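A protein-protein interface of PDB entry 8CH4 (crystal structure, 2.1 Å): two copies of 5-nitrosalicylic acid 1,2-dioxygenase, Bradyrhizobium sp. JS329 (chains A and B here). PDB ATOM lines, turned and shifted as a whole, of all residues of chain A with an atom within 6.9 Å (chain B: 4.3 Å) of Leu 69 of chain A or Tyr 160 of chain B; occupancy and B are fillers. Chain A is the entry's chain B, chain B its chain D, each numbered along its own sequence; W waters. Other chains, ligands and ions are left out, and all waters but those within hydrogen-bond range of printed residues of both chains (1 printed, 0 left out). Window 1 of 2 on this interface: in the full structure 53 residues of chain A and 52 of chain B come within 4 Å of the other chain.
O of Val 67 of chain A lies within hydrogen-bond range of NH1 of Arg 162 of chain B. NE of Arg 162 of chain B lies within hydrogen-bond range of O of Asn 28 of chain A (2.9 Å). O of Gly 68 of chain A lies within hydrogen-bond range of NH2 of Arg 162 of chain B (3.2 Å).
The backbone carbonyl oxygen (O) of Tyr 160 of chain B is in hydrogen-bond range of the guanidinium group (NH1) of Arg 162 of chain B, at 2.8 Å. O of Lys 24 of chain A lies close to OE1 of Gln 27 of chain A (3.3 Å). OG1 of Thr 72 of chain A sits at hydrogen-bond distance from O of Leu 69 of chain A, at 2.6 Å. The backbone carbonyl oxygen (O) of Val 25 of chain A sits close to the side-chain amide oxygen (OE1) of Gln 27 of chain A (3.1 Å). NE2 of Gln 27 of chain A sits close to N of Gly 70 of chain A, at 3.0 Å.
Among the printed residues, merely in contact across the chains: Phe 21 of chain A with Ile 75 of chain B, Val 25 of chain A with Ile 75 of chain B, Val 25 of chain A with Ala 156 of chain B, Val 25 of chain A with Ala 159 of chain B, Val 25 of chain A with Tyr 160 of chain B, Gln 27 of chain A with Ala 159 of chain B, Gln 27 of chain A with Tyr 160 of chain B, Gln 27 of chain A with Arg 162 of chain B, Thr 30 of chain A with Arg 162 of chain B, Asp 66 of chain A with Arg 162 of chain B, Leu 69 of chain A with Tyr 160 of chain B, Pro 79 of chain A with Tyr 160 of chain B, Pro 79 of chain A with Met 161 of chain B and Pro 79 of chain A with Arg 162 of chain B.
Of chain B, only Tyr 160 comes within 4 Å of Leu 69 of chain A. Tyr 160 of chain B touches just these residues of chain A: Val 25, Gln 27, Leu 69 and Pro 79. Of the printed residues of chain B, Phe 21 of chain A touches Ile 75 (3.4 Å). Of the printed residues of chain A, Ala 156 of chain B touches Val 25. Printed residues of chain B within 4 Å of Asn 28 of chain A: Arg 162 (2.9 Å). Of the printed residues of chain B, Pro 79 of chain A touches Tyr 160 (3.4 Å), Met 161 (3.9 Å) and Arg 162 (3.8 Å). Of the printed residues of chain A, Arg 162 of chain B touches Gln 27 (3.4 Å), Asn 28 (2.9 Å), Thr 30 (3.6 Å), Asp 66 (3.7 Å), Val 67 (3.4 Å), Gly 68 (3.2 Å) and Pro 79 (3.8 Å). Leu 157 of chain B touches none of the printed residues of chain A. Gly 80 of chain A touches none of the printed residues of chain B. The nearest printed residue of chain B that does not touch Leu 69 of chain A is Arg 162 of chain B (4.3 Å). The nearest printed residue of chain B that does not touch Asn 28 of chain A is Ala 159 of chain B (6.3 Å).
Of the 9 printed residues of chain B, 6 touch a printed residue of chain A. Among the printed residues, no Asp or Glu carboxylate lies within 4 Å of a Lys or Arg side-chain nitrogen of the other chain.
Position printed for both chains: 160. Of the 17 pairs that touch across the chains among the printed residues, none has its exchanged pair printed and touching as well.
Water W1 lies within hydrogen-bond range of the backbone carbonyl oxygen of Ala 159 of chain B (2.6 Å) and the backbone NH of Gln 27 of chain A (2.8 Å).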
ATOM      1  N   PHE A  21      40.381  11.740   2.230  1.00  0.00           N
ATOM      2  CA  PHE A  21      39.217  11.605   3.095  1.00  0.00           C
ATOM      3  C   PHE A  21      38.434  12.917   3.135  1.00  0.00           C
ATOM      4  O   PHE A  21      37.214  12.928   2.936  1.00  0.00           O
ATOM      5  CB  PHE A  21      39.598  11.161   4.511  1.00  0.00           C
ATOM      6  CG  PHE A  21      38.431  10.846   5.427  1.00  0.00           C
ATOM      7  CD1 PHE A  21      37.713   9.658   5.300  1.00  0.00           C
ATOM      8  CD2 PHE A  21      38.070  11.711   6.451  1.00  0.00           C
ATOM      9  CE1 PHE A  21      36.647   9.360   6.146  1.00  0.00           C
ATOM     10  CE2 PHE A  21      37.012  11.411   7.299  1.00  0.00           C
ATOM     11  CZ  PHE A  21      36.296  10.237   7.149  1.00  0.00           C
ATOM     12  N   LYS A  24      36.441  14.199   0.284  1.00  0.00           N
ATOM     13  CA  LYS A  24      35.276  13.375   0.001  1.00  0.00           C
ATOM     14  C   LYS A  24      34.269  13.444   1.143  1.00  0.00           C
ATOM     15  O   LYS A  24      33.093  13.153   0.936  1.00  0.00           O
ATOM     16  CB  LYS A  24      35.662  11.944  -0.390  1.00  0.00           C
ATOM     17  CG  LYS A  24      36.463  11.841  -1.687  1.00  0.00           C
ATOM     18  CD  LYS A  24      36.963  10.452  -2.038  1.00  0.00           C
ATOM     19  CE  LYS A  24      35.954   9.578  -2.761  1.00  0.00           C
ATOM     20  NZ  LYS A  24      36.308   8.144  -2.629  1.00  0.00           N
ATOM     21  N   VAL A  25      34.705  13.879   2.330  1.00  0.00           N
ATOM     22  CA  VAL A  25      33.798  13.840   3.468  1.00  0.00           C
ATOM     23  C   VAL A  25      32.964  15.123   3.552  1.00  0.00           C
ATOM     24  O   VAL A  25      31.808  15.086   3.983  1.00  0.00           O
ATOM     25  CB  VAL A  25      34.526  13.491   4.779  1.00  0.00           C
ATOM     26  CG1 VAL A  25      35.312  14.666   5.341  1.00  0.00           C
ATOM     27  CG2 VAL A  25      33.562  12.944   5.813  1.00  0.00           C
ATOM     28  N   ILE A  26      33.554  16.251   3.127  1.00  0.00           N
ATOM     29  CA  ILE A  26      32.897  17.549   3.221  1.00  0.00           C
ATOM     30  C   ILE A  26      31.930  17.748   2.049  1.00  0.00           C
ATOM     31  O   ILE A  26      32.309  17.749   0.875  1.00  0.00           O
ATOM     32  CB  ILE A  26      33.891  18.726   3.362  1.00  0.00           C
ATOM     33  CG1 ILE A  26      34.972  18.479   4.421  1.00  0.00           C
ATOM     34  CG2 ILE A  26      33.136  20.018   3.642  1.00  0.00           C
ATOM     35  CD1 ILE A  26      34.471  18.532   5.862  1.00  0.00           C
ATOM     36  N   GLN A  27      30.676  18.021   2.408  1.00  0.00           N
ATOM     37  CA  GLN A  27      29.604  18.150   1.449  1.00  0.00           C
ATOM     38  C   GLN A  27      29.402  19.620   1.083  1.00  0.00           C
ATOM     39  O   GLN A  27      29.857  20.526   1.788  1.00  0.00           O
ATOM     40  CB  GLN A  27      28.351  17.532   2.077  1.00  0.00           C
ATOM     41  CG  GLN A  27      28.509  16.051   2.439  1.00  0.00           C
ATOM     42  CD  GLN A  27      29.101  15.230   1.312  1.00  0.00           C
ATOM     43  OE1 GLN A  27      30.129  14.562   1.471  1.00  0.00           O
ATOM     44  NE2 GLN A  27      28.473  15.296   0.146  1.00  0.00           N
ATOM     45  N   ASN A  28      28.689  19.843  -0.027  1.00  0.00           N
ATOM     46  CA  ASN A  28      28.134  21.143  -0.347  1.00  0.00           C
ATOM     47  C   ASN A  28      26.973  21.426   0.597  1.00  0.00           C
ATOM     48  O   ASN A  28      26.349  20.511   1.125  1.00  0.00           O
ATOM     49  CB  ASN A  28      27.617  21.204  -1.779  1.00  0.00           C
ATOM     50  CG  ASN A  28      28.735  21.332  -2.788  1.00  0.00           C
ATOM     51  OD1 ASN A  28      29.447  22.335  -2.807  1.00  0.00           O
ATOM     52  ND2 ASN A  28      28.882  20.337  -3.644  1.00  0.00           N
ATOM     53  N   THR A  30      23.094  22.956   1.174  1.00  0.00           N
ATOM     54  CA  THR A  30      21.870  22.542   0.519  1.00  0.00           C
ATOM     55  C   THR A  30      20.871  23.697   0.513  1.00  0.00           C
ATOM     56  O   THR A  30      20.420  24.124   1.573  1.00  0.00           O
ATOM     57  CB  THR A  30      21.281  21.310   1.223  1.00  0.00           C
ATOM     58  OG1 THR A  30      20.611  21.704   2.424  1.00  0.00           O
ATOM     59  CG2 THR A  30      22.319  20.255   1.522  1.00  0.00           C
ATOM     60  N   GLU A  65      17.244  17.429  -4.363  1.00  0.00           N
ATOM     61  CA  GLU A  65      18.383  16.920  -5.124  1.00  0.00           C
ATOM     62  C   GLU A  65      19.726  17.426  -4.600  1.00  0.00           C
ATOM     63  O   GLU A  65      20.728  16.737  -4.765  1.00  0.00           O
ATOM     64  CB  GLU A  65      18.272  17.226  -6.618  1.00  0.00           C
ATOM     65  CG  GLU A  65      16.994  16.695  -7.233  1.00  0.00           C
ATOM     66  CD  GLU A  65      17.212  15.982  -8.555  1.00  0.00           C
ATOM     67  OE1 GLU A  65      17.924  16.565  -9.412  1.00  0.00           O
ATOM     68  OE2 GLU A  65      16.691  14.832  -8.710  1.00  0.00           O
ATOM     69  N   ASP A  66      19.752  18.620  -3.992  1.00  0.00           N
ATOM     70  CA  ASP A  66      20.981  19.193  -3.444  1.00  0.00           C
ATOM     71  C   ASP A  66      21.558  18.331  -2.316  1.00  0.00           C
ATOM     72  O   ASP A  66      22.733  18.450  -1.984  1.00  0.00           O
ATOM     73  CB  ASP A  66      20.706  20.555  -2.798  1.00  0.00           C
ATOM     74  CG  ASP A  66      20.721  21.764  -3.712  1.00  0.00           C
ATOM     75  OD1 ASP A  66      20.611  21.583  -4.933  1.00  0.00           O
ATOM     76  OD2 ASP A  66      20.808  22.892  -3.172  1.00  0.00           O
ATOM     77  N   VAL A  67      20.715  17.494  -1.700  1.00  0.00           N
ATOM     78  CA  VAL A  67      21.042  16.776  -0.481  1.00  0.00           C
ATOM     79  C   VAL A  67      21.971  15.601  -0.787  1.00  0.00           C
ATOM     80  O   VAL A  67      22.419  14.929   0.134  1.00  0.00           O
ATOM     81  CB  VAL A  67      19.748  16.354   0.243  1.00  0.00           C
ATOM     82  CG1 VAL A  67      19.738  14.923   0.755  1.00  0.00           C
ATOM     83  CG2 VAL A  67      19.323  17.352   1.309  1.00  0.00           C
ATOM     84  N   GLY A  68      22.296  15.377  -2.067  1.00  0.00           N
ATOM     85  CA  GLY A  68      23.156  14.269  -2.470  1.00  0.00           C
ATOM     86  C   GLY A  68      24.573  14.373  -1.900  1.00  0.00           C
ATOM     87  O   GLY A  68      24.988  15.451  -1.467  1.00  0.00           O
ATOM     88  N   LEU A  69      25.294  13.237  -1.893  1.00  0.00           N
ATOM     89  CA  LEU A  69      26.695  13.162  -1.488  1.00  0.00           C
ATOM     90  C   LEU A  69      27.593  13.283  -2.719  1.00  0.00           C
ATOM     91  O   LEU A  69      27.276  12.749  -3.780  1.00  0.00           O
ATOM     92  CB  LEU A  69      26.947  11.844  -0.742  1.00  0.00           C
ATOM     93  CG  LEU A  69      26.897  11.909   0.789  1.00  0.00           C
ATOM     94  CD1 LEU A  69      25.550  12.403   1.320  1.00  0.00           C
ATOM     95  CD2 LEU A  69      27.233  10.560   1.395  1.00  0.00           C
ATOM     96  N   GLY A  70      28.724  13.981  -2.576  1.00  0.00           N
ATOM     97  CA  GLY A  70      29.513  14.350  -3.739  1.00  0.00           C
ATOM     98  C   GLY A  70      28.681  15.233  -4.665  1.00  0.00           C
ATOM     99  O   GLY A  70      27.827  15.985  -4.199  1.00  0.00           O
ATOM    100  N   GLU A  71      28.920  15.131  -5.974  1.00  0.00           N
ATOM    101  CA  GLU A  71      28.115  15.875  -6.932  1.00  0.00           C
ATOM    102  C   GLU A  71      27.041  14.955  -7.512  1.00  0.00           C
ATOM    103  O   GLU A  71      27.071  14.633  -8.698  1.00  0.00           O
ATOM    104  CB  GLU A  71      28.984  16.504  -8.002  1.00  0.00           C
ATOM    105  N   THR A  72      26.099  14.522  -6.659  1.00  0.00           N
ATOM    106  CA  THR A  72      25.068  13.578  -7.066  1.00  0.00           C
ATOM    107  C   THR A  72      23.686  14.027  -6.583  1.00  0.00           C
ATOM    108  O   THR A  72      23.551  14.840  -5.665  1.00  0.00           O
ATOM    109  CB  THR A  72      25.387  12.141  -6.626  1.00  0.00           C
ATOM    110  OG1 THR A  72      25.196  12.031  -5.215  1.00  0.00           O
ATOM    111  CG2 THR A  72      26.770  11.681  -7.028  1.00  0.00           C
ATOM    112  N   LYS A  73      22.659  13.456  -7.225  1.00  0.00           N
ATOM    113  CA  LYS A  73      21.278  13.755  -6.906  1.00  0.00           C
ATOM    114  C   LYS A  73      20.910  13.083  -5.582  1.00  0.00           C
ATOM    115  O   LYS A  73      21.057  11.875  -5.415  1.00  0.00           O
ATOM    116  CB  LYS A  73      20.368  13.408  -8.093  1.00  0.00           C
ATOM    117  N   GLY A  74      20.450  13.893  -4.630  1.00  0.00           N
ATOM    118  CA  GLY A  74      20.005  13.368  -3.352  1.00  0.00           C
ATOM    119  C   GLY A  74      18.609  12.760  -3.437  1.00  0.00           C
ATOM    120  O   GLY A  74      17.856  13.041  -4.367  1.00  0.00           O
ATOM    121  N   PRO A  79      19.145  15.817   4.346  1.00  0.00           N
ATOM    122  CA  PRO A  79      20.145  14.739   4.370  1.00  0.00           C
ATOM    123  C   PRO A  79      19.729  13.498   5.169  1.00  0.00           C
ATOM    124  O   PRO A  79      19.972  12.365   4.751  1.00  0.00           O
ATOM    125  CB  PRO A  79      21.351  15.450   4.988  1.00  0.00           C
ATOM    126  CG  PRO A  79      21.199  16.885   4.523  1.00  0.00           C
ATOM    127  CD  PRO A  79      19.716  17.144   4.652  1.00  0.00           C
ATOM    128  N   GLY A  80      19.040  13.709   6.299  1.00  0.00           N
ATOM    129  CA  GLY A  80      18.723  12.605   7.193  1.00  0.00           C
ATOM    130  C   GLY A  80      17.223  12.339   7.339  1.00  0.00           C
ATOM    131  O   GLY A  80      16.841  11.495   8.141  1.00  0.00           O
ATOM    132  N   TYR A 160      21.024   2.375   3.715  1.00  0.00           N
ATOM    133  CA  TYR A 160      22.393   2.856   3.556  1.00  0.00           C
ATOM    134  C   TYR A 160      23.345   2.086   4.475  1.00  0.00           C
ATOM    135  O   TYR A 160      24.503   1.841   4.143  1.00  0.00           O
ATOM    136  CB  TYR A 160      22.452   4.370   3.806  1.00  0.00           C
ATOM    137  CG  TYR A 160      21.744   5.284   2.819  1.00  0.00           C
ATOM    138  CD1 TYR A 160      21.391   4.865   1.542  1.00  0.00           C
ATOM    139  CD2 TYR A 160      21.473   6.608   3.147  1.00  0.00           C
ATOM    140  CE1 TYR A 160      20.778   5.721   0.639  1.00  0.00           C
ATOM    141  CE2 TYR A 160      20.861   7.480   2.258  1.00  0.00           C
ATOM    142  CZ  TYR A 160      20.515   7.035   0.996  1.00  0.00           C
ATOM    143  OH  TYR A 160      19.905   7.879   0.113  1.00  0.00           O
ATOM    144  N   ILE B  75      34.095   5.728   2.200  1.00  0.00           N
ATOM    145  CA  ILE B  75      35.187   6.205   3.042  1.00  0.00           C
ATOM    146  C   ILE B  75      34.942   5.852   4.515  1.00  0.00           C
ATOM    147  O   ILE B  75      35.739   6.202   5.387  1.00  0.00           O
ATOM    148  CB  ILE B  75      35.405   7.717   2.838  1.00  0.00           C
ATOM    149  CG1 ILE B  75      34.105   8.507   3.006  1.00  0.00           C
ATOM    150  CG2 ILE B  75      36.078   7.987   1.500  1.00  0.00           C
ATOM    151  CD1 ILE B  75      34.302   9.974   3.327  1.00  0.00           C
ATOM    152  N   PHE B  82      33.596   5.255  11.138  1.00  0.00           N
ATOM    153  CA  PHE B  82      34.742   5.819  10.443  1.00  0.00           C
ATOM    154  C   PHE B  82      35.969   5.690  11.327  1.00  0.00           C
ATOM    155  O   PHE B  82      35.862   5.823  12.544  1.00  0.00           O
ATOM    156  CB  PHE B  82      34.430   7.270  10.081  1.00  0.00           C
ATOM    157  CG  PHE B  82      33.154   7.346   9.291  1.00  0.00           C
ATOM    158  CD1 PHE B  82      31.919   7.328   9.938  1.00  0.00           C
ATOM    159  CD2 PHE B  82      33.189   7.328   7.903  1.00  0.00           C
ATOM    160  CE1 PHE B  82      30.735   7.343   9.211  1.00  0.00           C
ATOM    161  CE2 PHE B  82      32.003   7.354   7.179  1.00  0.00           C
ATOM    162  CZ  PHE B  82      30.783   7.362   7.832  1.00  0.00           C
ATOM    163  N   ALA B 156      32.223  12.086   9.880  1.00  0.00           N
ATOM    164  CA  ALA B 156      31.611  11.959   8.568  1.00  0.00           C
ATOM    165  C   ALA B 156      30.086  11.919   8.691  1.00  0.00           C
ATOM    166  O   ALA B 156      29.398  12.501   7.856  1.00  0.00           O
ATOM    167  CB  ALA B 156      32.200  10.789   7.814  1.00  0.00           C
ATOM    168  N   LEU B 157      29.565  11.301   9.767  1.00  0.00           N
ATOM    169  CA  LEU B 157      28.133  11.333  10.041  1.00  0.00           C
ATOM    170  C   LEU B 157      27.667  12.782   9.998  1.00  0.00           C
ATOM    171  O   LEU B 157      26.783  13.141   9.238  1.00  0.00           O
ATOM    172  CB  LEU B 157      27.846  10.722  11.416  1.00  0.00           C
ATOM    173  CG  LEU B 157      27.082   9.392  11.415  1.00  0.00           C
ATOM    174  CD1 LEU B 157      27.840   8.321  10.640  1.00  0.00           C
ATOM    175  CD2 LEU B 157      26.794   8.918  12.844  1.00  0.00           C
ATOM    176  N   LEU B 158      28.343  13.619  10.775  1.00  0.00           N
ATOM    177  CA  LEU B 158      27.994  15.016  10.927  1.00  0.00           C
ATOM    178  C   LEU B 158      28.224  15.780   9.632  1.00  0.00           C
ATOM    179  O   LEU B 158      27.373  16.575   9.262  1.00  0.00           O
ATOM    180  CB  LEU B 158      28.784  15.568  12.109  1.00  0.00           C
ATOM    181  CG  LEU B 158      28.246  15.063  13.448  1.00  0.00           C
ATOM    182  CD1 LEU B 158      29.124  15.548  14.593  1.00  0.00           C
ATOM    183  CD2 LEU B 158      26.793  15.515  13.633  1.00  0.00           C
ATOM    184  N   ALA B 159      29.313  15.474   8.916  1.00  0.00           N
ATOM    185  CA  ALA B 159      29.623  16.162   7.669  1.00  0.00           C
ATOM    186  C   ALA B 159      28.464  16.014   6.685  1.00  0.00           C
ATOM    187  O   ALA B 159      28.061  16.985   6.067  1.00  0.00           O
ATOM    188  CB  ALA B 159      30.917  15.645   7.081  1.00  0.00           C
ATOM    189  N   TYR B 160      27.910  14.800   6.588  1.00  0.00           N
ATOM    190  CA  TYR B 160      26.855  14.459   5.647  1.00  0.00           C
ATOM    191  C   TYR B 160      25.538  15.158   6.001  1.00  0.00           C
ATOM    192  O   TYR B 160      24.757  15.466   5.099  1.00  0.00           O
ATOM    193  CB  TYR B 160      26.604  12.944   5.658  1.00  0.00           C
ATOM    194  CG  TYR B 160      27.729  12.053   5.179  1.00  0.00           C
ATOM    195  CD1 TYR B 160      28.802  12.575   4.465  1.00  0.00           C
ATOM    196  CD2 TYR B 160      27.703  10.672   5.397  1.00  0.00           C
ATOM    197  CE1 TYR B 160      29.824  11.762   4.002  1.00  0.00           C
ATOM    198  CE2 TYR B 160      28.723   9.842   4.948  1.00  0.00           C
ATOM    199  CZ  TYR B 160      29.780  10.395   4.234  1.00  0.00           C
ATOM    200  OH  TYR B 160      30.811   9.632   3.762  1.00  0.00           O
ATOM    201  N   MET B 161      25.253  15.313   7.309  1.00  0.00           N
ATOM    202  CA  MET B 161      24.060  15.989   7.789  1.00  0.00           C
ATOM    203  C   MET B 161      24.250  17.498   7.661  1.00  0.00           C
ATOM    204  O   MET B 161      23.330  18.259   7.938  1.00  0.00           O
ATOM    205  CB  MET B 161      23.829  15.713   9.274  1.00  0.00           C
ATOM    206  CG  MET B 161      23.257  14.363   9.582  1.00  0.00           C
ATOM    207  SD  MET B 161      23.172  14.122  11.395  1.00  0.00           S
ATOM    208  CE  MET B 161      22.000  15.392  11.886  1.00  0.00           C
ATOM    209  N   ARG B 162      25.469  17.912   7.303  1.00  0.00           N
ATOM    210  CA  ARG B 162      25.896  19.304   7.290  1.00  0.00           C
ATOM    211  C   ARG B 162      25.729  19.903   8.684  1.00  0.00           C
ATOM    212  O   ARG B 162      25.336  21.060   8.814  1.00  0.00           O
ATOM    213  CB  ARG B 162      25.122  20.137   6.256  1.00  0.00           C
ATOM    214  CG  ARG B 162      25.476  19.877   4.799  1.00  0.00           C
ATOM    215  CD  ARG B 162      25.017  18.516   4.306  1.00  0.00           C
ATOM    216  NE  ARG B 162      25.228  18.527   2.875  1.00  0.00           N
ATOM    217  CZ  ARG B 162      24.917  17.557   2.023  1.00  0.00           C
ATOM    218  NH1 ARG B 162      24.395  16.412   2.446  1.00  0.00           N
ATOM    219  NH2 ARG B 162      25.167  17.738   0.739  1.00  0.00           N
HETATM  220  O   HOH W   1      29.763  18.596   4.949  1.00  0.00           O
